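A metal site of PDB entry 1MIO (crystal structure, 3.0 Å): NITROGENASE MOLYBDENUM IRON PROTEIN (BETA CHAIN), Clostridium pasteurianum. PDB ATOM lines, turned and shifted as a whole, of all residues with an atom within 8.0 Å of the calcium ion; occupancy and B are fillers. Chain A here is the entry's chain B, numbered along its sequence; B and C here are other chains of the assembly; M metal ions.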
ATOM      1  N   GLY A 297      -3.641 -17.229  28.268  1.00  0.00           N
ATOM      2  CA  GLY A 297      -2.809 -17.531  27.123  1.00  0.00           C
ATOM      3  C   GLY A 297      -1.852 -18.665  27.363  1.00  0.00           C
ATOM      4  O   GLY A 297      -1.618 -19.498  26.504  1.00  0.00           O
ATOM      5  N   GLN A 298      -1.251 -18.617  28.555  1.00  0.00           N
ATOM      6  CA  GLN A 298      -0.305 -19.616  28.999  1.00  0.00           C
ATOM      7  C   GLN A 298      -0.995 -20.950  29.149  1.00  0.00           C
ATOM      8  O   GLN A 298      -0.390 -21.965  28.858  1.00  0.00           O
ATOM      9  CB  GLN A 298       0.291 -19.204  30.343  1.00  0.00           C
ATOM     10  CG  GLN A 298       1.110 -17.922  30.273  1.00  0.00           C
ATOM     11  CD  GLN A 298       1.749 -17.579  31.595  1.00  0.00           C
ATOM     12  OE1 GLN A 298       1.140 -17.544  32.661  1.00  0.00           O
ATOM     13  NE2 GLN A 298       3.030 -17.306  31.508  1.00  0.00           N
ATOM     14  N   ILE A 300      -3.740 -22.073  27.239  1.00  0.00           N
ATOM     15  CA  ILE A 300      -3.945 -22.529  25.849  1.00  0.00           C
ATOM     16  C   ILE A 300      -2.608 -22.922  25.252  1.00  0.00           C
ATOM     17  O   ILE A 300      -2.477 -23.993  24.673  1.00  0.00           O
ATOM     18  CB  ILE A 300      -4.572 -21.417  25.005  1.00  0.00           C
ATOM     19  CG1 ILE A 300      -5.919 -21.012  25.594  1.00  0.00           C
ATOM     20  CG2 ILE A 300      -4.721 -21.882  23.563  1.00  0.00           C
ATOM     21  CD1 ILE A 300      -7.074 -22.009  25.543  1.00  0.00           C
ATOM     22  N   ASP A 301      -1.570 -22.143  25.430  1.00  0.00           N
ATOM     23  CA  ASP A 301      -0.255 -22.504  24.999  1.00  0.00           C
ATOM     24  C   ASP A 301       0.181 -23.826  25.600  1.00  0.00           C
ATOM     25  O   ASP A 301       0.798 -24.586  24.848  1.00  0.00           O
ATOM     26  CB  ASP A 301       0.681 -21.397  25.386  1.00  0.00           C
ATOM     27  CG  ASP A 301       2.127 -21.606  24.977  1.00  0.00           C
ATOM     28  OD1 ASP A 301       2.442 -21.668  23.786  1.00  0.00           O
ATOM     29  OD2 ASP A 301       2.935 -21.696  25.873  1.00  0.00           O
ATOM     30  N   LEU A 302      -0.060 -24.161  26.876  1.00  0.00           N
ATOM     31  CA  LEU A 302       0.401 -25.412  27.521  1.00  0.00           C
ATOM     32  C   LEU A 302      -0.406 -26.578  27.009  1.00  0.00           C
ATOM     33  O   LEU A 302       0.172 -27.633  26.769  1.00  0.00           O
ATOM     34  CB  LEU A 302       0.260 -25.367  29.082  1.00  0.00           C
ATOM     35  CG  LEU A 302       0.483 -26.568  30.027  1.00  0.00           C
ATOM     36  CD1 LEU A 302       1.828 -27.219  29.870  1.00  0.00           C
ATOM     37  CD2 LEU A 302       0.377 -26.049  31.401  1.00  0.00           C
ATOM     38  N   ILE A 304      -1.681 -26.697  24.032  1.00  0.00           N
ATOM     39  CA  ILE A 304      -1.205 -26.798  22.663  1.00  0.00           C
ATOM     40  C   ILE A 304       0.180 -27.417  22.629  1.00  0.00           C
ATOM     41  O   ILE A 304       0.421 -28.287  21.796  1.00  0.00           O
ATOM     42  CB  ILE A 304      -1.303 -25.349  22.019  1.00  0.00           C
ATOM     43  CG1 ILE A 304      -2.654 -25.231  21.324  1.00  0.00           C
ATOM     44  CG2 ILE A 304      -0.240 -25.065  20.977  1.00  0.00           C
ATOM     45  CD1 ILE A 304      -2.962 -23.819  20.851  1.00  0.00           C
ATOM     46  N   ASP A 305       1.147 -27.099  23.482  1.00  0.00           N
ATOM     47  CA  ASP A 305       2.464 -27.762  23.497  1.00  0.00           C
ATOM     48  C   ASP A 305       2.468 -29.257  23.916  1.00  0.00           C
ATOM     49  O   ASP A 305       3.164 -30.079  23.310  1.00  0.00           O
ATOM     50  CB  ASP A 305       3.456 -27.048  24.445  1.00  0.00           C
ATOM     51  CG  ASP A 305       3.779 -25.592  24.202  1.00  0.00           C
ATOM     52  OD1 ASP A 305       3.587 -25.108  23.082  1.00  0.00           O
ATOM     53  OD2 ASP A 305       4.211 -24.964  25.154  1.00  0.00           O
ATOM     54  N   ALA A 306       1.685 -29.632  24.957  1.00  0.00           N
ATOM     55  CA  ALA A 306       1.490 -31.010  25.433  1.00  0.00           C
ATOM     56  C   ALA A 306       0.485 -31.794  24.621  1.00  0.00           C
ATOM     57  O   ALA A 306       0.321 -32.982  24.874  1.00  0.00           O
ATOM     58  CB  ALA A 306       1.004 -31.043  26.881  1.00  0.00           C
ATOM     59  N   SER B  57      14.702 -23.350  23.068  1.00  0.00           N
ATOM     60  CA  SER B  57      13.355 -23.831  22.700  1.00  0.00           C
ATOM     61  C   SER B  57      12.933 -25.161  23.402  1.00  0.00           C
ATOM     62  O   SER B  57      11.851 -25.265  23.984  1.00  0.00           O
ATOM     63  CB  SER B  57      13.303 -23.949  21.128  1.00  0.00           C
ATOM     64  OG  SER B  57      13.660 -22.755  20.424  1.00  0.00           O
ATOM     65  N   PHE B  60      12.172 -24.492  27.180  1.00  0.00           N
ATOM     66  CA  PHE B  60      10.980 -23.693  27.488  1.00  0.00           C
ATOM     67  C   PHE B  60       9.758 -23.957  26.592  1.00  0.00           C
ATOM     68  O   PHE B  60       8.666 -23.391  26.782  1.00  0.00           O
ATOM     69  CB  PHE B  60      11.321 -22.208  27.422  1.00  0.00           C
ATOM     70  CG  PHE B  60      12.437 -21.722  28.326  1.00  0.00           C
ATOM     71  CD1 PHE B  60      13.739 -21.761  27.877  1.00  0.00           C
ATOM     72  CD2 PHE B  60      12.160 -21.237  29.572  1.00  0.00           C
ATOM     73  CE1 PHE B  60      14.768 -21.337  28.673  1.00  0.00           C
ATOM     74  CE2 PHE B  60      13.198 -20.811  30.371  1.00  0.00           C
ATOM     75  CZ  PHE B  60      14.497 -20.855  29.931  1.00  0.00           C
ATOM     76  N   LYS B  61       9.883 -24.843  25.598  1.00  0.00           N
ATOM     77  CA  LYS B  61       8.872 -25.151  24.587  1.00  0.00           C
ATOM     78  C   LYS B  61       8.348 -23.779  24.070  1.00  0.00           C
ATOM     79  O   LYS B  61       7.149 -23.366  24.107  1.00  0.00           O
ATOM     80  CB  LYS B  61       7.789 -26.077  25.238  1.00  0.00           C
ATOM     81  CG  LYS B  61       8.215 -27.506  25.697  1.00  0.00           C
ATOM     82  CD  LYS B  61       8.615 -28.609  24.638  1.00  0.00           C
ATOM     83  CE  LYS B  61      10.089 -28.726  24.000  1.00  0.00           C
ATOM     84  NZ  LYS B  61      10.309 -29.611  22.836  1.00  0.00           N
ATOM     85  N   GLU B  62       9.365 -23.016  23.638  1.00  0.00           N
ATOM     86  CA  GLU B  62       9.271 -21.583  23.348  1.00  0.00           C
ATOM     87  C   GLU B  62      10.229 -21.199  22.205  1.00  0.00           C
ATOM     88  O   GLU B  62      10.997 -22.074  21.786  1.00  0.00           O
ATOM     89  CB  GLU B  62       9.603 -20.836  24.641  1.00  0.00           C
ATOM     90  CG  GLU B  62       8.820 -19.612  25.034  1.00  0.00           C
ATOM     91  CD  GLU B  62       7.304 -19.763  25.082  1.00  0.00           C
ATOM     92  OE1 GLU B  62       6.815 -20.675  25.753  1.00  0.00           O
ATOM     93  OE2 GLU B  62       6.627 -18.936  24.489  1.00  0.00           O
ATOM     94  N   PRO B  63      10.191 -19.974  21.612  1.00  0.00           N
ATOM     95  CA  PRO B  63      11.167 -19.527  20.631  1.00  0.00           C
ATOM     96  C   PRO B  63      12.327 -18.710  21.175  1.00  0.00           C
ATOM     97  O   PRO B  63      12.119 -17.757  21.926  1.00  0.00           O
ATOM     98  CB  PRO B  63      10.359 -18.749  19.598  1.00  0.00           C
ATOM     99  CG  PRO B  63       8.900 -18.860  19.982  1.00  0.00           C
ATOM    100  CD  PRO B  63       9.005 -19.126  21.453  1.00  0.00           C
ATOM    101  N   LEU B 208      10.337 -15.836  27.943  1.00  0.00           N
ATOM    102  CA  LEU B 208      10.489 -17.300  27.750  1.00  0.00           C
ATOM    103  C   LEU B 208       9.543 -18.301  28.417  1.00  0.00           C
ATOM    104  O   LEU B 208       9.808 -19.434  28.755  1.00  0.00           O
ATOM    105  CB  LEU B 208      11.961 -17.644  28.048  1.00  0.00           C
ATOM    106  CG  LEU B 208      12.999 -17.126  27.050  1.00  0.00           C
ATOM    107  CD1 LEU B 208      14.401 -17.463  27.457  1.00  0.00           C
ATOM    108  CD2 LEU B 208      12.662 -17.743  25.720  1.00  0.00           C
ATOM    109  N   ASP B 209       8.320 -17.828  28.438  1.00  0.00           N
ATOM    110  CA  ASP B 209       7.090 -18.475  28.834  1.00  0.00           C
ATOM    111  C   ASP B 209       6.033 -17.584  28.153  1.00  0.00           C
ATOM    112  O   ASP B 209       6.333 -16.639  27.396  1.00  0.00           O
ATOM    113  CB  ASP B 209       6.836 -18.392  30.310  1.00  0.00           C
ATOM    114  CG  ASP B 209       6.903 -16.973  30.830  1.00  0.00           C
ATOM    115  OD1 ASP B 209       7.956 -16.386  30.689  1.00  0.00           O
ATOM    116  OD2 ASP B 209       5.911 -16.467  31.349  1.00  0.00           O
ATOM    117  N   GLY B 210       4.754 -17.850  28.359  1.00  0.00           N
ATOM    118  CA  GLY B 210       3.824 -16.900  27.797  1.00  0.00           C
ATOM    119  C   GLY B 210       2.833 -17.489  26.823  1.00  0.00           C
ATOM    120  O   GLY B 210       2.834 -18.706  26.579  1.00  0.00           O
ATOM    121  N   PRO B 211       1.953 -16.565  26.385  1.00  0.00           N
ATOM    122  CA  PRO B 211       0.648 -16.825  25.831  1.00  0.00           C
ATOM    123  C   PRO B 211       0.599 -17.286  24.412  1.00  0.00           C
ATOM    124  O   PRO B 211       1.347 -16.706  23.654  1.00  0.00           O
ATOM    125  CB  PRO B 211      -0.120 -15.533  25.987  1.00  0.00           C
ATOM    126  CG  PRO B 211       0.675 -14.708  26.964  1.00  0.00           C
ATOM    127  CD  PRO B 211       2.085 -15.110  26.586  1.00  0.00           C
ATOM    128  N   THR B 212      -0.161 -18.270  23.978  1.00  0.00           N
ATOM    129  CA  THR B 212      -0.389 -18.405  22.566  1.00  0.00           C
ATOM    130  C   THR B 212      -1.609 -17.475  22.453  1.00  0.00           C
ATOM    131  O   THR B 212      -2.583 -17.709  23.167  1.00  0.00           O
ATOM    132  CB  THR B 212      -0.657 -19.873  22.225  1.00  0.00           C
ATOM    133  OG1 THR B 212       0.625 -20.477  22.068  1.00  0.00           O
ATOM    134  CG2 THR B 212      -1.429 -20.096  20.959  1.00  0.00           C
ATOM    135  N   TYR B 417       6.361 -30.808  30.618  1.00  0.00           N
ATOM    136  CA  TYR B 417       5.652 -29.586  30.253  1.00  0.00           C
ATOM    137  C   TYR B 417       5.044 -28.842  31.449  1.00  0.00           C
ATOM    138  O   TYR B 417       4.437 -29.455  32.303  1.00  0.00           O
ATOM    139  CB  TYR B 417       4.518 -29.913  29.252  1.00  0.00           C
ATOM    140  CG  TYR B 417       4.945 -30.561  27.928  1.00  0.00           C
ATOM    141  CD1 TYR B 417       5.167 -31.924  27.865  1.00  0.00           C
ATOM    142  CD2 TYR B 417       5.093 -29.813  26.783  1.00  0.00           C
ATOM    143  CE1 TYR B 417       5.517 -32.536  26.680  1.00  0.00           C
ATOM    144  CE2 TYR B 417       5.439 -30.417  25.602  1.00  0.00           C
ATOM    145  CZ  TYR B 417       5.631 -31.766  25.578  1.00  0.00           C
ATOM    146  OH  TYR B 417       5.868 -32.363  24.392  1.00  0.00           O
ATOM    147  N   TYR B 420       8.203 -24.419  33.852  1.00  0.00           N
ATOM    148  CA  TYR B 420       8.779 -23.079  33.759  1.00  0.00           C
ATOM    149  C   TYR B 420       7.801 -22.059  34.351  1.00  0.00           C
ATOM    150  O   TYR B 420       8.097 -20.860  34.349  1.00  0.00           O
ATOM    151  CB  TYR B 420       9.142 -22.727  32.242  1.00  0.00           C
ATOM    152  CG  TYR B 420       8.372 -23.510  31.190  1.00  0.00           C
ATOM    153  CD1 TYR B 420       7.043 -23.239  30.973  1.00  0.00           C
ATOM    154  CD2 TYR B 420       8.935 -24.627  30.575  1.00  0.00           C
ATOM    155  CE1 TYR B 420       6.286 -24.085  30.170  1.00  0.00           C
ATOM    156  CE2 TYR B 420       8.188 -25.486  29.779  1.00  0.00           C
ATOM    157  CZ  TYR B 420       6.855 -25.194  29.589  1.00  0.00           C
ATOM    158  OH  TYR B 420       6.043 -26.012  28.826  1.00  0.00           O
ATOM    159  N   TYR B 421       6.656 -22.559  34.851  1.00  0.00           N
ATOM    160  CA  TYR B 421       5.623 -21.732  35.443  1.00  0.00           C
ATOM    161  C   TYR B 421       5.699 -21.848  36.972  1.00  0.00           C
ATOM    162  O   TYR B 421       5.037 -21.110  37.708  1.00  0.00           O
ATOM    163  CB  TYR B 421       4.222 -22.145  34.916  1.00  0.00           C
ATOM    164  CG  TYR B 421       3.876 -21.997  33.413  1.00  0.00           C
ATOM    165  CD1 TYR B 421       4.436 -21.012  32.601  1.00  0.00           C
ATOM    166  CD2 TYR B 421       2.984 -22.877  32.808  1.00  0.00           C
ATOM    167  CE1 TYR B 421       4.109 -20.919  31.253  1.00  0.00           C
ATOM    168  CE2 TYR B 421       2.658 -22.798  31.464  1.00  0.00           C
ATOM    169  CZ  TYR B 421       3.221 -21.809  30.669  1.00  0.00           C
ATOM    170  OH  TYR B 421       2.924 -21.718  29.304  1.00  0.00           O
ATOM    171  N   PHE C 468       7.881 -23.562  17.301  1.00  0.00           N
ATOM    172  CA  PHE C 468       7.092 -22.701  18.182  1.00  0.00           C
ATOM    173  C   PHE C 468       6.758 -21.345  17.638  1.00  0.00           C
ATOM    174  O   PHE C 468       5.999 -20.641  18.256  1.00  0.00           O
ATOM    175  CB  PHE C 468       7.799 -22.577  19.510  1.00  0.00           C
ATOM    176  CG  PHE C 468       7.913 -23.951  20.162  1.00  0.00           C
ATOM    177  CD1 PHE C 468       6.784 -24.656  20.499  1.00  0.00           C
ATOM    178  CD2 PHE C 468       9.165 -24.514  20.365  1.00  0.00           C
ATOM    179  CE1 PHE C 468       6.913 -25.914  21.022  1.00  0.00           C
ATOM    180  CE2 PHE C 468       9.258 -25.779  20.896  1.00  0.00           C
ATOM    181  CZ  PHE C 468       8.135 -26.474  21.217  1.00  0.00           C
ATOM    182  N   GLN C 471       3.467 -22.547  15.362  1.00  0.00           N
ATOM    183  CA  GLN C 471       2.471 -22.969  16.329  1.00  0.00           C
ATOM    184  C   GLN C 471       1.804 -21.808  17.092  1.00  0.00           C
ATOM    185  O   GLN C 471       0.596 -21.836  17.297  1.00  0.00           O
ATOM    186  CB  GLN C 471       3.197 -23.922  17.265  1.00  0.00           C
ATOM    187  CG  GLN C 471       2.451 -25.173  17.744  1.00  0.00           C
ATOM    188  CD  GLN C 471       2.448 -26.298  16.732  1.00  0.00           C
ATOM    189  OE1 GLN C 471       1.468 -26.964  16.375  1.00  0.00           O
ATOM    190  NE2 GLN C 471       3.638 -26.523  16.206  1.00  0.00           N
ATOM    191  N   LYS C 472       2.558 -20.752  17.436  1.00  0.00           N
ATOM    192  CA  LYS C 472       2.162 -19.533  18.187  1.00  0.00           C
ATOM    193  C   LYS C 472       1.207 -18.572  17.499  1.00  0.00           C
ATOM    194  O   LYS C 472       0.477 -17.798  18.124  1.00  0.00           O
ATOM    195  CB  LYS C 472       3.374 -18.762  18.527  1.00  0.00           C
ATOM    196  CG  LYS C 472       3.349 -18.101  19.861  1.00  0.00           C
ATOM    197  CD  LYS C 472       4.617 -18.625  20.523  1.00  0.00           C
ATOM    198  CE  LYS C 472       4.815 -18.232  21.955  1.00  0.00           C
ATOM    199  NZ  LYS C 472       3.683 -18.692  22.739  1.00  0.00           N
HETATM  200 CA    CA M   1       5.089 -22.618  24.736  1.00  0.00          CA
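OD1 of Asp 301 is in salt-bridge range of NZ of Lys 472 of chain C, at 3.4 Å.
OE2 of Glu 62 of chain B is in salt-bridge range of NZ of Lys 472 of chain C (3.4 Å).
OD2 of Asp 301 sits close to OH of Tyr 421 of chain B (3.4 Å).
The side-chain carboxylate of Asp 301 is in hydrogen-bond range of the side-chain hydroxyl of Thr 212 of chain B (2.8 Å).
The side-chain hydroxyl (OG) of Ser 57 of chain B lies close to the backbone carbonyl oxygen (O) of Glu 62 of chain B, at 3.1 Å.
O of Lys 61 of chain B is bound to the calcium ion (2.3 Å).
OD2 of Asp 305 binds the calcium ion, 2.5 Å away.
The calcium ion is bound by the side-chain carboxylate (OD2) of Asp 301.
The calcium ion is bound by OE1 of Glu 62 of chain B (2.8 Å).
Slightly farther from the calcium ion lies OD1 of Asp 301 (3.0 Å).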
